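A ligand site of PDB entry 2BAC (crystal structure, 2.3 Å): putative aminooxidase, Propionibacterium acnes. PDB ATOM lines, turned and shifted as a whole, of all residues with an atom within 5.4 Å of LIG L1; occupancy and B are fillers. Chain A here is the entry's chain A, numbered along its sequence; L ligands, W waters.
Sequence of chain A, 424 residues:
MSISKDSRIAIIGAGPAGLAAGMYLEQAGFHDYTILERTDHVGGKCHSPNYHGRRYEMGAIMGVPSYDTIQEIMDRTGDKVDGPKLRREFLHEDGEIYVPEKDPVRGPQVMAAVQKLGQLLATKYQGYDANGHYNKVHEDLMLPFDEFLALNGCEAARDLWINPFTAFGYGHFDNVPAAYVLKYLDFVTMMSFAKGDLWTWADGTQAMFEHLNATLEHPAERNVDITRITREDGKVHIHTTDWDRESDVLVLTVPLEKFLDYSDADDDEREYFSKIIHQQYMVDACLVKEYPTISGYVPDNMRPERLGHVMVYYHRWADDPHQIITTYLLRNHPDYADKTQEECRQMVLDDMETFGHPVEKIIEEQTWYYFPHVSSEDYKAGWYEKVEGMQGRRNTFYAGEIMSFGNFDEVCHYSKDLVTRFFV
O1 of LIG L1 sits at hydrogen-bond distance from OH of Tyr 297 (2.5 Å). NE of Arg 88 lies within salt-bridge range of O1 of LIG L1 (2.7 Å). The backbone NH (N) of Arg 87 lies close to an oxygen (O2) of LIG L1 (3.4 Å). The side-chain hydroxyl of Tyr 67 sits at hydrogen-bond distance from an oxygen (O7) of LG2 L2 (2.9 Å). The backbone NH (N) of Met 62 lies within hydrogen-bond range of an oxygen (O8) of LG2 L2 (3.1 Å). The backbone carbonyl oxygen (O) of Met 62 is in hydrogen-bond range of a nitrogen (N7) of LG2 L2, at 2.9 Å. The backbone NH of Ile 61 lies within hydrogen-bond range of an oxygen (O8) of LG2 L2, at 3.4 Å. O10 of LG2 L2 is in hydrogen-bond range of N of Asn 407 (3.2 Å).
NH2 of Arg 88 sits close to O of Phe 193 (3.3 Å). O of Phe 168 lies within hydrogen-bond range of OH of Tyr 370 (2.7 Å). The backbone carbonyl oxygen (O) of Ala 167 lies within hydrogen-bond range of the side-chain hydroxyl (OH) of Tyr 281 (2.8 Å). O of Arg 87 is in hydrogen-bond range of N of Ser 295, at 3.1 Å. The backbone carbonyl oxygen (O) of Val 312 lies within hydrogen-bond range of the backbone NH (N) of Tyr 328. The side-chain hydroxyl (OH) of Tyr 170 sits close to the side-chain hydroxyl (OH) of Tyr 370 (3.3 Å). The side-chain hydroxyl (OG) of Ser 295 is in hydrogen-bond range of the backbone NH (N) of His 315, 2.9 Å away.
Merely in contact with LIG L1: Tyr 67, Phe 168, Tyr 184, Tyr 281, Val 312, Tyr 170, Met 62, Tyr 370, Leu 86, Ile 61, Ser 295, Tyr 314, Val 64, Tyr 328 and Gly 63. 18 residues have an atom within 4 Å of LIG L1: Ile 61, Met 62, Gly 63, Val 64, Tyr 67, Leu 86, Arg 87, Arg 88, Phe 168, Tyr 170, Tyr 184, Tyr 281, Ser 295, Tyr 297, Val 312, Tyr 314, Tyr 328 and Tyr 370.
Water W1 lies within hydrogen-bond range of O2 of LIG L1, NH2 of Arg 88 and O of Leu 86.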
ATOM      1  N   ILE A  61     -25.355  -2.123   8.737  1.00  0.00           N
ATOM      2  CA  ILE A  61     -24.342  -3.163   8.595  1.00  0.00           C
ATOM      3  C   ILE A  61     -24.505  -4.364   9.538  1.00  0.00           C
ATOM      4  O   ILE A  61     -24.281  -5.530   9.147  1.00  0.00           O
ATOM      5  CB  ILE A  61     -22.992  -2.588   8.891  1.00  0.00           C
ATOM      6  CG1 ILE A  61     -22.649  -1.491   7.881  1.00  0.00           C
ATOM      7  CG2 ILE A  61     -21.950  -3.720   8.981  1.00  0.00           C
ATOM      8  CD1 ILE A  61     -21.499  -0.611   8.337  1.00  0.00           C
ATOM      9  N   MET A  62     -24.861  -4.068  10.781  1.00  0.00           N
ATOM     10  CA  MET A  62     -24.637  -5.006  11.865  1.00  0.00           C
ATOM     11  C   MET A  62     -25.799  -5.079  12.864  1.00  0.00           C
ATOM     12  O   MET A  62     -26.733  -4.266  12.840  1.00  0.00           O
ATOM     13  CB  MET A  62     -23.351  -4.607  12.589  1.00  0.00           C
ATOM     14  CG  MET A  62     -23.530  -3.565  13.654  1.00  0.00           C
ATOM     15  SD  MET A  62     -21.994  -2.980  14.349  1.00  0.00           S
ATOM     16  CE  MET A  62     -21.247  -2.156  12.923  1.00  0.00           C
ATOM     17  N   GLY A  63     -25.702  -6.078  13.740  1.00  0.00           N
ATOM     18  CA  GLY A  63     -26.629  -6.274  14.848  1.00  0.00           C
ATOM     19  C   GLY A  63     -25.917  -6.947  16.018  1.00  0.00           C
ATOM     20  O   GLY A  63     -24.734  -7.273  15.928  1.00  0.00           O
ATOM     21  N   VAL A  64     -26.628  -7.117  17.125  1.00  0.00           N
ATOM     22  CA  VAL A  64     -26.110  -7.837  18.304  1.00  0.00           C
ATOM     23  C   VAL A  64     -27.073  -8.985  18.644  1.00  0.00           C
ATOM     24  O   VAL A  64     -28.229  -8.942  18.235  1.00  0.00           O
ATOM     25  CB  VAL A  64     -25.937  -6.869  19.530  1.00  0.00           C
ATOM     26  CG1 VAL A  64     -24.837  -5.869  19.256  1.00  0.00           C
ATOM     27  CG2 VAL A  64     -27.211  -6.122  19.844  1.00  0.00           C
ATOM     28  N   TYR A  67     -30.854  -8.644  19.452  1.00  0.00           N
ATOM     29  CA  TYR A  67     -31.807  -8.278  18.397  1.00  0.00           C
ATOM     30  C   TYR A  67     -32.894  -9.346  18.171  1.00  0.00           C
ATOM     31  O   TYR A  67     -32.964  -9.965  17.098  1.00  0.00           O
ATOM     32  CB  TYR A  67     -31.042  -8.071  17.071  1.00  0.00           C
ATOM     33  CG  TYR A  67     -30.474  -6.703  16.845  1.00  0.00           C
ATOM     34  CD1 TYR A  67     -30.084  -5.878  17.898  1.00  0.00           C
ATOM     35  CD2 TYR A  67     -30.298  -6.233  15.536  1.00  0.00           C
ATOM     36  CE1 TYR A  67     -29.564  -4.588  17.631  1.00  0.00           C
ATOM     37  CE2 TYR A  67     -29.779  -4.966  15.285  1.00  0.00           C
ATOM     38  CZ  TYR A  67     -29.420  -4.160  16.319  1.00  0.00           C
ATOM     39  OH  TYR A  67     -28.917  -2.905  16.013  1.00  0.00           O
ATOM     40  N   LEU A  86     -16.389  -8.518  12.047  1.00  0.00           N
ATOM     41  CA  LEU A  86     -16.034  -7.132  12.351  1.00  0.00           C
ATOM     42  C   LEU A  86     -14.825  -7.077  13.282  1.00  0.00           C
ATOM     43  O   LEU A  86     -14.814  -7.724  14.330  1.00  0.00           O
ATOM     44  CB  LEU A  86     -17.222  -6.427  12.997  1.00  0.00           C
ATOM     45  CG  LEU A  86     -18.449  -6.127  12.119  1.00  0.00           C
ATOM     46  CD1 LEU A  86     -19.590  -5.642  12.984  1.00  0.00           C
ATOM     47  CD2 LEU A  86     -18.148  -5.117  11.004  1.00  0.00           C
ATOM     48  N   ARG A  87     -13.806  -6.319  12.889  1.00  0.00           N
ATOM     49  CA  ARG A  87     -12.619  -6.083  13.709  1.00  0.00           C
ATOM     50  C   ARG A  87     -12.196  -4.625  13.570  1.00  0.00           C
ATOM     51  O   ARG A  87     -12.306  -4.051  12.498  1.00  0.00           O
ATOM     52  CB  ARG A  87     -11.471  -6.983  13.215  1.00  0.00           C
ATOM     53  CG  ARG A  87     -11.505  -8.392  13.710  1.00  0.00           C
ATOM     54  CD  ARG A  87     -10.922  -9.327  12.684  1.00  0.00           C
ATOM     55  NE  ARG A  87     -10.180 -10.472  13.241  1.00  0.00           N
ATOM     56  CZ  ARG A  87     -10.680 -11.414  14.042  1.00  0.00           C
ATOM     57  NH1 ARG A  87      -9.879 -12.424  14.437  1.00  0.00           N
ATOM     58  NH2 ARG A  87     -11.946 -11.373  14.464  1.00  0.00           N
ATOM     59  N   ARG A  88     -11.671  -4.044  14.647  1.00  0.00           N
ATOM     60  CA  ARG A  88     -11.375  -2.610  14.667  1.00  0.00           C
ATOM     61  C   ARG A  88     -10.022  -2.268  15.299  1.00  0.00           C
ATOM     62  O   ARG A  88      -9.583  -2.917  16.228  1.00  0.00           O
ATOM     63  CB  ARG A  88     -12.453  -1.857  15.452  1.00  0.00           C
ATOM     64  CG  ARG A  88     -12.587  -2.272  16.932  1.00  0.00           C
ATOM     65  CD  ARG A  88     -13.712  -1.514  17.619  1.00  0.00           C
ATOM     66  NE  ARG A  88     -15.026  -2.145  17.432  1.00  0.00           N
ATOM     67  CZ  ARG A  88     -15.607  -3.030  18.263  1.00  0.00           C
ATOM     68  NH1 ARG A  88     -15.000  -3.440  19.400  1.00  0.00           N
ATOM     69  NH2 ARG A  88     -16.806  -3.513  17.959  1.00  0.00           N
ATOM     70  N   ALA A 167     -19.654   8.220  16.278  1.00  0.00           N
ATOM     71  CA  ALA A 167     -19.073   7.685  15.010  1.00  0.00           C
ATOM     72  C   ALA A 167     -20.123   7.014  14.100  1.00  0.00           C
ATOM     73  O   ALA A 167     -20.016   7.046  12.848  1.00  0.00           O
ATOM     74  CB  ALA A 167     -17.945   6.696  15.326  1.00  0.00           C
ATOM     75  N   PHE A 168     -21.124   6.393  14.745  1.00  0.00           N
ATOM     76  CA  PHE A 168     -22.203   5.700  14.065  1.00  0.00           C
ATOM     77  C   PHE A 168     -23.371   6.651  13.705  1.00  0.00           C
ATOM     78  O   PHE A 168     -24.477   6.189  13.386  1.00  0.00           O
ATOM     79  CB  PHE A 168     -22.741   4.550  14.963  1.00  0.00           C
ATOM     80  CG  PHE A 168     -21.854   3.323  15.005  1.00  0.00           C
ATOM     81  CD1 PHE A 168     -20.495   3.376  14.663  1.00  0.00           C
ATOM     82  CD2 PHE A 168     -22.389   2.099  15.418  1.00  0.00           C
ATOM     83  CE1 PHE A 168     -19.688   2.230  14.719  1.00  0.00           C
ATOM     84  CE2 PHE A 168     -21.612   0.946  15.476  1.00  0.00           C
ATOM     85  CZ  PHE A 168     -20.253   0.999  15.134  1.00  0.00           C
ATOM     86  N   TYR A 170     -25.153   9.034  15.359  1.00  0.00           N
ATOM     87  CA  TYR A 170     -26.244   9.363  16.274  1.00  0.00           C
ATOM     88  C   TYR A 170     -26.100  10.708  17.020  1.00  0.00           C
ATOM     89  O   TYR A 170     -26.998  11.079  17.793  1.00  0.00           O
ATOM     90  CB  TYR A 170     -26.460   8.213  17.237  1.00  0.00           C
ATOM     91  CG  TYR A 170     -27.005   6.967  16.565  1.00  0.00           C
ATOM     92  CD1 TYR A 170     -28.251   6.994  15.914  1.00  0.00           C
ATOM     93  CD2 TYR A 170     -26.297   5.759  16.589  1.00  0.00           C
ATOM     94  CE1 TYR A 170     -28.758   5.842  15.269  1.00  0.00           C
ATOM     95  CE2 TYR A 170     -26.796   4.614  15.978  1.00  0.00           C
ATOM     96  CZ  TYR A 170     -28.030   4.660  15.318  1.00  0.00           C
ATOM     97  OH  TYR A 170     -28.528   3.527  14.713  1.00  0.00           O
ATOM     98  N   TYR A 184     -30.649   2.264  23.001  1.00  0.00           N
ATOM     99  CA  TYR A 184     -29.770   1.616  22.022  1.00  0.00           C
ATOM    100  C   TYR A 184     -28.620   0.914  22.771  1.00  0.00           C
ATOM    101  O   TYR A 184     -28.624  -0.302  22.923  1.00  0.00           O
ATOM    102  CB  TYR A 184     -29.286   2.659  21.015  1.00  0.00           C
ATOM    103  CG  TYR A 184     -28.043   2.344  20.217  1.00  0.00           C
ATOM    104  CD1 TYR A 184     -27.804   1.078  19.705  1.00  0.00           C
ATOM    105  CD2 TYR A 184     -27.134   3.354  19.911  1.00  0.00           C
ATOM    106  CE1 TYR A 184     -26.677   0.800  18.954  1.00  0.00           C
ATOM    107  CE2 TYR A 184     -26.000   3.104  19.150  1.00  0.00           C
ATOM    108  CZ  TYR A 184     -25.766   1.812  18.676  1.00  0.00           C
ATOM    109  OH  TYR A 184     -24.643   1.556  17.945  1.00  0.00           O
ATOM    110  N   THR A 189     -26.001  -4.579  25.348  1.00  0.00           N
ATOM    111  CA  THR A 189     -25.611  -4.250  23.993  1.00  0.00           C
ATOM    112  C   THR A 189     -24.212  -3.635  23.949  1.00  0.00           C
ATOM    113  O   THR A 189     -23.398  -3.990  23.095  1.00  0.00           O
ATOM    114  CB  THR A 189     -26.628  -3.311  23.348  1.00  0.00           C
ATOM    115  OG1 THR A 189     -27.901  -3.970  23.309  1.00  0.00           O
ATOM    116  CG2 THR A 189     -26.228  -2.944  21.912  1.00  0.00           C
ATOM    117  N   PHE A 193     -20.990  -5.236  21.946  1.00  0.00           N
ATOM    118  CA  PHE A 193     -20.143  -4.460  21.043  1.00  0.00           C
ATOM    119  C   PHE A 193     -18.698  -4.489  21.525  1.00  0.00           C
ATOM    120  O   PHE A 193     -17.802  -4.826  20.764  1.00  0.00           O
ATOM    121  CB  PHE A 193     -20.648  -3.004  20.903  1.00  0.00           C
ATOM    122  CG  PHE A 193     -19.758  -2.154  20.049  1.00  0.00           C
ATOM    123  CD1 PHE A 193     -19.982  -2.047  18.677  1.00  0.00           C
ATOM    124  CD2 PHE A 193     -18.652  -1.485  20.608  1.00  0.00           C
ATOM    125  CE1 PHE A 193     -19.118  -1.269  17.865  1.00  0.00           C
ATOM    126  CE2 PHE A 193     -17.776  -0.711  19.817  1.00  0.00           C
ATOM    127  CZ  PHE A 193     -18.017  -0.591  18.438  1.00  0.00           C
ATOM    128  N   LEU A 198     -20.808  -9.332  17.289  1.00  0.00           N
ATOM    129  CA  LEU A 198     -21.608  -8.541  16.349  1.00  0.00           C
ATOM    130  C   LEU A 198     -22.014  -9.337  15.089  1.00  0.00           C
ATOM    131  O   LEU A 198     -21.180  -9.988  14.454  1.00  0.00           O
ATOM    132  CB  LEU A 198     -20.825  -7.271  15.954  1.00  0.00           C
ATOM    133  CG  LEU A 198     -20.478  -6.327  17.114  1.00  0.00           C
ATOM    134  CD1 LEU A 198     -19.446  -5.282  16.678  1.00  0.00           C
ATOM    135  CD2 LEU A 198     -21.729  -5.639  17.694  1.00  0.00           C
ATOM    136  N   TYR A 281     -26.085  12.251   8.221  1.00  0.00           N
ATOM    137  CA  TYR A 281     -25.019  11.240   8.286  1.00  0.00           C
ATOM    138  C   TYR A 281     -24.618  10.835   6.850  1.00  0.00           C
ATOM    139  O   TYR A 281     -25.467  10.361   6.062  1.00  0.00           O
ATOM    140  CB  TYR A 281     -25.542  10.049   9.101  1.00  0.00           C
ATOM    141  CG  TYR A 281     -24.535   9.015   9.569  1.00  0.00           C
ATOM    142  CD1 TYR A 281     -23.252   9.377   9.977  1.00  0.00           C
ATOM    143  CD2 TYR A 281     -24.908   7.656   9.655  1.00  0.00           C
ATOM    144  CE1 TYR A 281     -22.341   8.413  10.418  1.00  0.00           C
ATOM    145  CE2 TYR A 281     -24.008   6.686  10.111  1.00  0.00           C
ATOM    146  CZ  TYR A 281     -22.729   7.079  10.489  1.00  0.00           C
ATOM    147  OH  TYR A 281     -21.822   6.136  10.935  1.00  0.00           O
ATOM    148  N   SER A 295     -10.923  -2.436  10.230  1.00  0.00           N
ATOM    149  CA  SER A 295     -11.718  -1.208  10.282  1.00  0.00           C
ATOM    150  C   SER A 295     -11.083  -0.237  11.259  1.00  0.00           C
ATOM    151  O   SER A 295     -10.395  -0.651  12.192  1.00  0.00           O
ATOM    152  CB  SER A 295     -13.164  -1.523  10.662  1.00  0.00           C
ATOM    153  OG  SER A 295     -13.791  -2.270   9.625  1.00  0.00           O
ATOM    154  N   TYR A 297     -11.629   3.348  13.681  1.00  0.00           N
ATOM    155  CA  TYR A 297     -12.365   4.389  14.403  1.00  0.00           C
ATOM    156  C   TYR A 297     -11.397   5.482  14.748  1.00  0.00           C
ATOM    157  O   TYR A 297     -10.232   5.206  15.017  1.00  0.00           O
ATOM    158  CB  TYR A 297     -12.910   3.871  15.724  1.00  0.00           C
ATOM    159  CG  TYR A 297     -14.075   2.924  15.607  1.00  0.00           C
ATOM    160  CD1 TYR A 297     -15.339   3.284  16.070  1.00  0.00           C
ATOM    161  CD2 TYR A 297     -13.914   1.666  15.028  1.00  0.00           C
ATOM    162  CE1 TYR A 297     -16.416   2.415  15.985  1.00  0.00           C
ATOM    163  CE2 TYR A 297     -14.987   0.799  14.908  1.00  0.00           C
ATOM    164  CZ  TYR A 297     -16.237   1.179  15.389  1.00  0.00           C
ATOM    165  OH  TYR A 297     -17.308   0.325  15.275  1.00  0.00           O
ATOM    166  N   VAL A 312     -15.137   7.020  11.354  1.00  0.00           N
ATOM    167  CA  VAL A 312     -14.913   5.572  11.240  1.00  0.00           C
ATOM    168  C   VAL A 312     -14.960   5.162   9.760  1.00  0.00           C
ATOM    169  O   VAL A 312     -15.542   5.856   8.928  1.00  0.00           O
ATOM    170  CB  VAL A 312     -16.005   4.784  12.024  1.00  0.00           C
ATOM    171  CG1 VAL A 312     -17.405   5.106  11.446  1.00  0.00           C
ATOM    172  CG2 VAL A 312     -15.734   3.261  12.004  1.00  0.00           C
ATOM    173  N   TYR A 313     -14.313   4.056   9.403  1.00  0.00           N
ATOM    174  CA  TYR A 313     -14.457   3.499   8.053  1.00  0.00           C
ATOM    175  C   TYR A 313     -14.494   1.991   8.101  1.00  0.00           C
ATOM    176  O   TYR A 313     -13.919   1.389   9.005  1.00  0.00           O
ATOM    177  CB  TYR A 313     -13.367   3.987   7.092  1.00  0.00           C
ATOM    178  CG  TYR A 313     -11.957   3.677   7.526  1.00  0.00           C
ATOM    179  CD1 TYR A 313     -11.392   2.422   7.335  1.00  0.00           C
ATOM    180  CD2 TYR A 313     -11.180   4.651   8.126  1.00  0.00           C
ATOM    181  CE1 TYR A 313     -10.084   2.155   7.751  1.00  0.00           C
ATOM    182  CE2 TYR A 313      -9.883   4.401   8.527  1.00  0.00           C
ATOM    183  CZ  TYR A 313      -9.340   3.167   8.342  1.00  0.00           C
ATOM    184  OH  TYR A 313      -8.033   2.959   8.769  1.00  0.00           O
ATOM    185  N   TYR A 314     -15.142   1.408   7.103  1.00  0.00           N
ATOM    186  CA  TYR A 314     -15.536   0.011   7.157  1.00  0.00           C
ATOM    187  C   TYR A 314     -14.761  -0.886   6.209  1.00  0.00           C
ATOM    188  O   TYR A 314     -14.847  -0.748   4.990  1.00  0.00           O
ATOM    189  CB  TYR A 314     -17.038  -0.104   6.887  1.00  0.00           C
ATOM    190  CG  TYR A 314     -17.635  -1.485   6.917  1.00  0.00           C
ATOM    191  CD1 TYR A 314     -17.119  -2.512   7.734  1.00  0.00           C
ATOM    192  CD2 TYR A 314     -18.774  -1.760   6.168  1.00  0.00           C
ATOM    193  CE1 TYR A 314     -17.708  -3.783   7.763  1.00  0.00           C
ATOM    194  CE2 TYR A 314     -19.386  -3.021   6.197  1.00  0.00           C
ATOM    195  CZ  TYR A 314     -18.848  -4.036   6.984  1.00  0.00           C
ATOM    196  OH  TYR A 314     -19.473  -5.272   6.948  1.00  0.00           O
ATOM    197  N   HIS A 315     -14.037  -1.829   6.809  1.00  0.00           N
ATOM    198  CA  HIS A 315     -13.311  -2.865   6.095  1.00  0.00           C
ATOM    199  C   HIS A 315     -14.187  -4.126   6.048  1.00  0.00           C
ATOM    200  O   HIS A 315     -14.247  -4.878   7.001  1.00  0.00           O
ATOM    201  CB  HIS A 315     -11.981  -3.143   6.809  1.00  0.00           C
ATOM    202  CG  HIS A 315     -11.125  -4.192   6.158  1.00  0.00           C
ATOM    203  ND1 HIS A 315     -10.905  -5.431   6.725  1.00  0.00           N
ATOM    204  CD2 HIS A 315     -10.430  -4.185   4.986  1.00  0.00           C
ATOM    205  CE1 HIS A 315     -10.113  -6.137   5.933  1.00  0.00           C
ATOM    206  NE2 HIS A 315      -9.805  -5.402   4.881  1.00  0.00           N
ATOM    207  N   TYR A 328     -17.545   7.230   7.074  1.00  0.00           N
ATOM    208  CA  TYR A 328     -18.687   7.780   7.821  1.00  0.00           C
ATOM    209  C   TYR A 328     -18.372   9.108   8.515  1.00  0.00           C
ATOM    210  O   TYR A 328     -17.390   9.206   9.272  1.00  0.00           O
ATOM    211  CB  TYR A 328     -19.198   6.743   8.836  1.00  0.00           C
ATOM    212  CG  TYR A 328     -19.516   5.426   8.184  1.00  0.00           C
ATOM    213  CD1 TYR A 328     -20.806   5.108   7.802  1.00  0.00           C
ATOM    214  CD2 TYR A 328     -18.485   4.520   7.875  1.00  0.00           C
ATOM    215  CE1 TYR A 328     -21.097   3.900   7.162  1.00  0.00           C
ATOM    216  CE2 TYR A 328     -18.748   3.307   7.240  1.00  0.00           C
ATOM    217  CZ  TYR A 328     -20.053   3.003   6.879  1.00  0.00           C
ATOM    218  OH  TYR A 328     -20.297   1.813   6.242  1.00  0.00           O
ATOM    219  N   TYR A 370     -31.318  10.765   9.164  1.00  0.00           N
ATOM    220  CA  TYR A 370     -30.810   9.833  10.146  1.00  0.00           C
ATOM    221  C   TYR A 370     -31.176  10.246  11.572  1.00  0.00           C
ATOM    222  O   TYR A 370     -31.228  11.444  11.893  1.00  0.00           O
ATOM    223  CB  TYR A 370     -29.295   9.741   9.975  1.00  0.00           C
ATOM    224  CG  TYR A 370     -28.643   8.546  10.655  1.00  0.00           C
ATOM    225  CD1 TYR A 370     -28.788   7.268  10.131  1.00  0.00           C
ATOM    226  CD2 TYR A 370     -27.872   8.705  11.804  1.00  0.00           C
ATOM    227  CE1 TYR A 370     -28.185   6.181  10.728  1.00  0.00           C
ATOM    228  CE2 TYR A 370     -27.263   7.622  12.407  1.00  0.00           C
ATOM    229  CZ  TYR A 370     -27.431   6.353  11.870  1.00  0.00           C
ATOM    230  OH  TYR A 370     -26.839   5.270  12.460  1.00  0.00           O
ATOM    231  N   ASN A 407     -32.317   2.566  14.969  1.00  0.00           N
ATOM    232  CA  ASN A 407     -31.723   1.294  14.493  1.00  0.00           C
ATOM    233  C   ASN A 407     -32.810   0.267  14.101  1.00  0.00           C
ATOM    234  O   ASN A 407     -33.967   0.409  14.487  1.00  0.00           O
ATOM    235  CB  ASN A 407     -30.648   0.742  15.470  1.00  0.00           C
ATOM    236  CG  ASN A 407     -31.211  -0.097  16.658  1.00  0.00           C
ATOM    237  OD1 ASN A 407     -32.150  -0.872  16.530  1.00  0.00           O
ATOM    238  ND2 ASN A 407     -30.552   0.041  17.809  1.00  0.00           N
HETATM  239  O1  LIG L   1     -16.147  -1.884  14.960  1.00  0.00           O
HETATM  240  C1  LIG L   1     -15.821  -2.859  14.265  1.00  0.00           C
HETATM  241  O2  LIG L   1     -15.242  -3.871  14.744  1.00  0.00           O
HETATM  242  C2  LIG L   1     -16.151  -2.784  12.802  1.00  0.00           C
HETATM  243  C3  LIG L   1     -17.048  -1.557  12.597  1.00  0.00           C
HETATM  244  C4  LIG L   1     -16.948  -1.008  11.173  1.00  0.00           C
HETATM  245  C5  LIG L   1     -17.382   0.448  11.151  1.00  0.00           C
HETATM  246  C6  LIG L   1     -18.781   0.537  10.582  1.00  0.00           C
HETATM  247  C7  LIG L   1     -19.441   1.867  10.853  1.00  0.00           C
HETATM  248  C8  LIG L   1     -20.868   1.648  11.324  1.00  0.00           C
HETATM  249  C9  LIG L   1     -21.689   2.804  10.793  1.00  0.00           C
HETATM  250  C10 LIG L   1     -23.057   3.048  11.419  1.00  0.00           C
HETATM  251  C11 LIG L   1     -23.638   2.051  12.400  1.00  0.00           C
HETATM  252  C12 LIG L   1     -24.811   2.466  12.860  1.00  0.00           C
HETATM  253  C13 LIG L   1     -25.704   1.817  13.821  1.00  0.00           C
HETATM  254  C14 LIG L   1     -25.521   0.674  14.440  1.00  0.00           C
HETATM  255  C15 LIG L   1     -26.589   0.279  15.350  1.00  0.00           C
HETATM  256  C16 LIG L   1     -26.534  -0.856  16.061  1.00  0.00           C
HETATM  257  C17 LIG L   1     -25.392  -1.851  15.993  1.00  0.00           C
HETATM  258  C18 LIG L   1     -25.663  -3.024  16.933  1.00  0.00           C
HETATM  259  P1  LG2 L   2     -36.114   3.858   6.987  1.00  0.00           P
HETATM  260  O1  LG2 L   2     -35.093   2.769   6.962  1.00  0.00           O
HETATM  261  O2  LG2 L   2     -35.522   5.245   6.865  1.00  0.00           O
HETATM  262  O3  LG2 L   2     -37.223   3.565   5.875  1.00  0.00           O
HETATM  263  C1  LG2 L   2     -38.352   4.404   5.641  1.00  0.00           C
HETATM  264  C2  LG2 L   2     -39.005   4.018   4.302  1.00  0.00           C
HETATM  265  O4  LG2 L   2     -40.093   4.880   4.029  1.00  0.00           O
HETATM  266  C3  LG2 L   2     -38.043   4.104   3.123  1.00  0.00           C
HETATM  267  O5  LG2 L   2     -38.103   2.971   2.264  1.00  0.00           O
HETATM  268  C4  LG2 L   2     -38.456   5.398   2.450  1.00  0.00           C
HETATM  269  O6  LG2 L   2     -38.193   5.450   1.060  1.00  0.00           O
HETATM  270  C5  LG2 L   2     -39.934   5.434   2.729  1.00  0.00           C
HETATM  271  N1  LG2 L   2     -40.545   6.768   2.619  1.00  0.00           N
HETATM  272  C6  LG2 L   2     -40.051   7.985   3.033  1.00  0.00           C
HETATM  273  N2  LG2 L   2     -40.967   8.939   2.728  1.00  0.00           N
HETATM  274  C7  LG2 L   2     -42.039   8.348   2.147  1.00  0.00           C
HETATM  275  C8  LG2 L   2     -43.247   8.860   1.644  1.00  0.00           C
HETATM  276  N3  LG2 L   2     -43.557  10.141   1.797  1.00  0.00           N
HETATM  277  N4  LG2 L   2     -44.152   7.985   1.094  1.00  0.00           N
HETATM  278  C9  LG2 L   2     -43.872   6.620   1.041  1.00  0.00           C
HETATM  279  N5  LG2 L   2     -42.680   6.121   1.538  1.00  0.00           N
HETATM  280  C10 LG2 L   2     -41.777   6.982   2.067  1.00  0.00           C
HETATM  281  N6  LG2 L   2     -29.212   0.093  12.198  1.00  0.00           N
HETATM  282  C11 LG2 L   2     -28.817  -1.048  12.868  1.00  0.00           C
HETATM  283  O7  LG2 L   2     -29.664  -1.645  13.531  1.00  0.00           O
HETATM  284  N7  LG2 L   2     -27.502  -1.492  12.799  1.00  0.00           N
HETATM  285  C12 LG2 L   2     -26.573  -0.814  12.033  1.00  0.00           C
HETATM  286  O8  LG2 L   2     -25.401  -1.227  11.978  1.00  0.00           O
HETATM  287  C13 LG2 L   2     -26.962   0.342  11.348  1.00  0.00           C
HETATM  288  N8  LG2 L   2     -26.053   1.104  10.641  1.00  0.00           N
HETATM  289  C14 LG2 L   2     -26.472   2.156   9.865  1.00  0.00           C
HETATM  290  C15 LG2 L   2     -25.543   2.797   9.045  1.00  0.00           C
HETATM  291  C16 LG2 L   2     -25.981   3.812   8.188  1.00  0.00           C
HETATM  292  C17 LG2 L   2     -24.983   4.505   7.296  1.00  0.00           C
HETATM  293  C18 LG2 L   2     -27.354   4.158   8.161  1.00  0.00           C
HETATM  294  C19 LG2 L   2     -27.882   5.245   7.254  1.00  0.00           C
HETATM  295  C20 LG2 L   2     -28.261   3.496   8.988  1.00  0.00           C
HETATM  296  C21 LG2 L   2     -27.827   2.502   9.851  1.00  0.00           C
HETATM  297  N9  LG2 L   2     -28.701   1.862  10.725  1.00  0.00           N
HETATM  298  C22 LG2 L   2     -28.283   0.771  11.432  1.00  0.00           C
HETATM  299  C23 LG2 L   2     -30.064   2.403  11.059  1.00  0.00           C
HETATM  300  C24 LG2 L   2     -31.185   1.615  10.374  1.00  0.00           C
HETATM  301  O9  LG2 L   2     -30.874   1.334   9.027  1.00  0.00           O
HETATM  302  C25 LG2 L   2     -32.485   2.396  10.475  1.00  0.00           C
HETATM  303  O10 LG2 L   2     -32.731   2.775  11.819  1.00  0.00           O
HETATM  304  C26 LG2 L   2     -33.688   1.589  10.009  1.00  0.00           C
HETATM  305  O11 LG2 L   2     -33.550   1.262   8.647  1.00  0.00           O
HETATM  306  C27 LG2 L   2     -34.945   2.413  10.210  1.00  0.00           C
HETATM  307  O12 LG2 L   2     -36.008   1.811   9.502  1.00  0.00           O
HETATM  308  P2  LG2 L   2     -37.355   2.622   9.240  1.00  0.00           P
HETATM  309  O13 LG2 L   2     -38.346   1.736   8.519  1.00  0.00           O
HETATM  310  O14 LG2 L   2     -37.823   3.146  10.573  1.00  0.00           O
HETATM  311  O15 LG2 L   2     -36.935   3.876   8.364  1.00  0.00           O
HETATM  312  O   HOH W   1     -15.361  -5.694  16.546  1.00  0.00           O
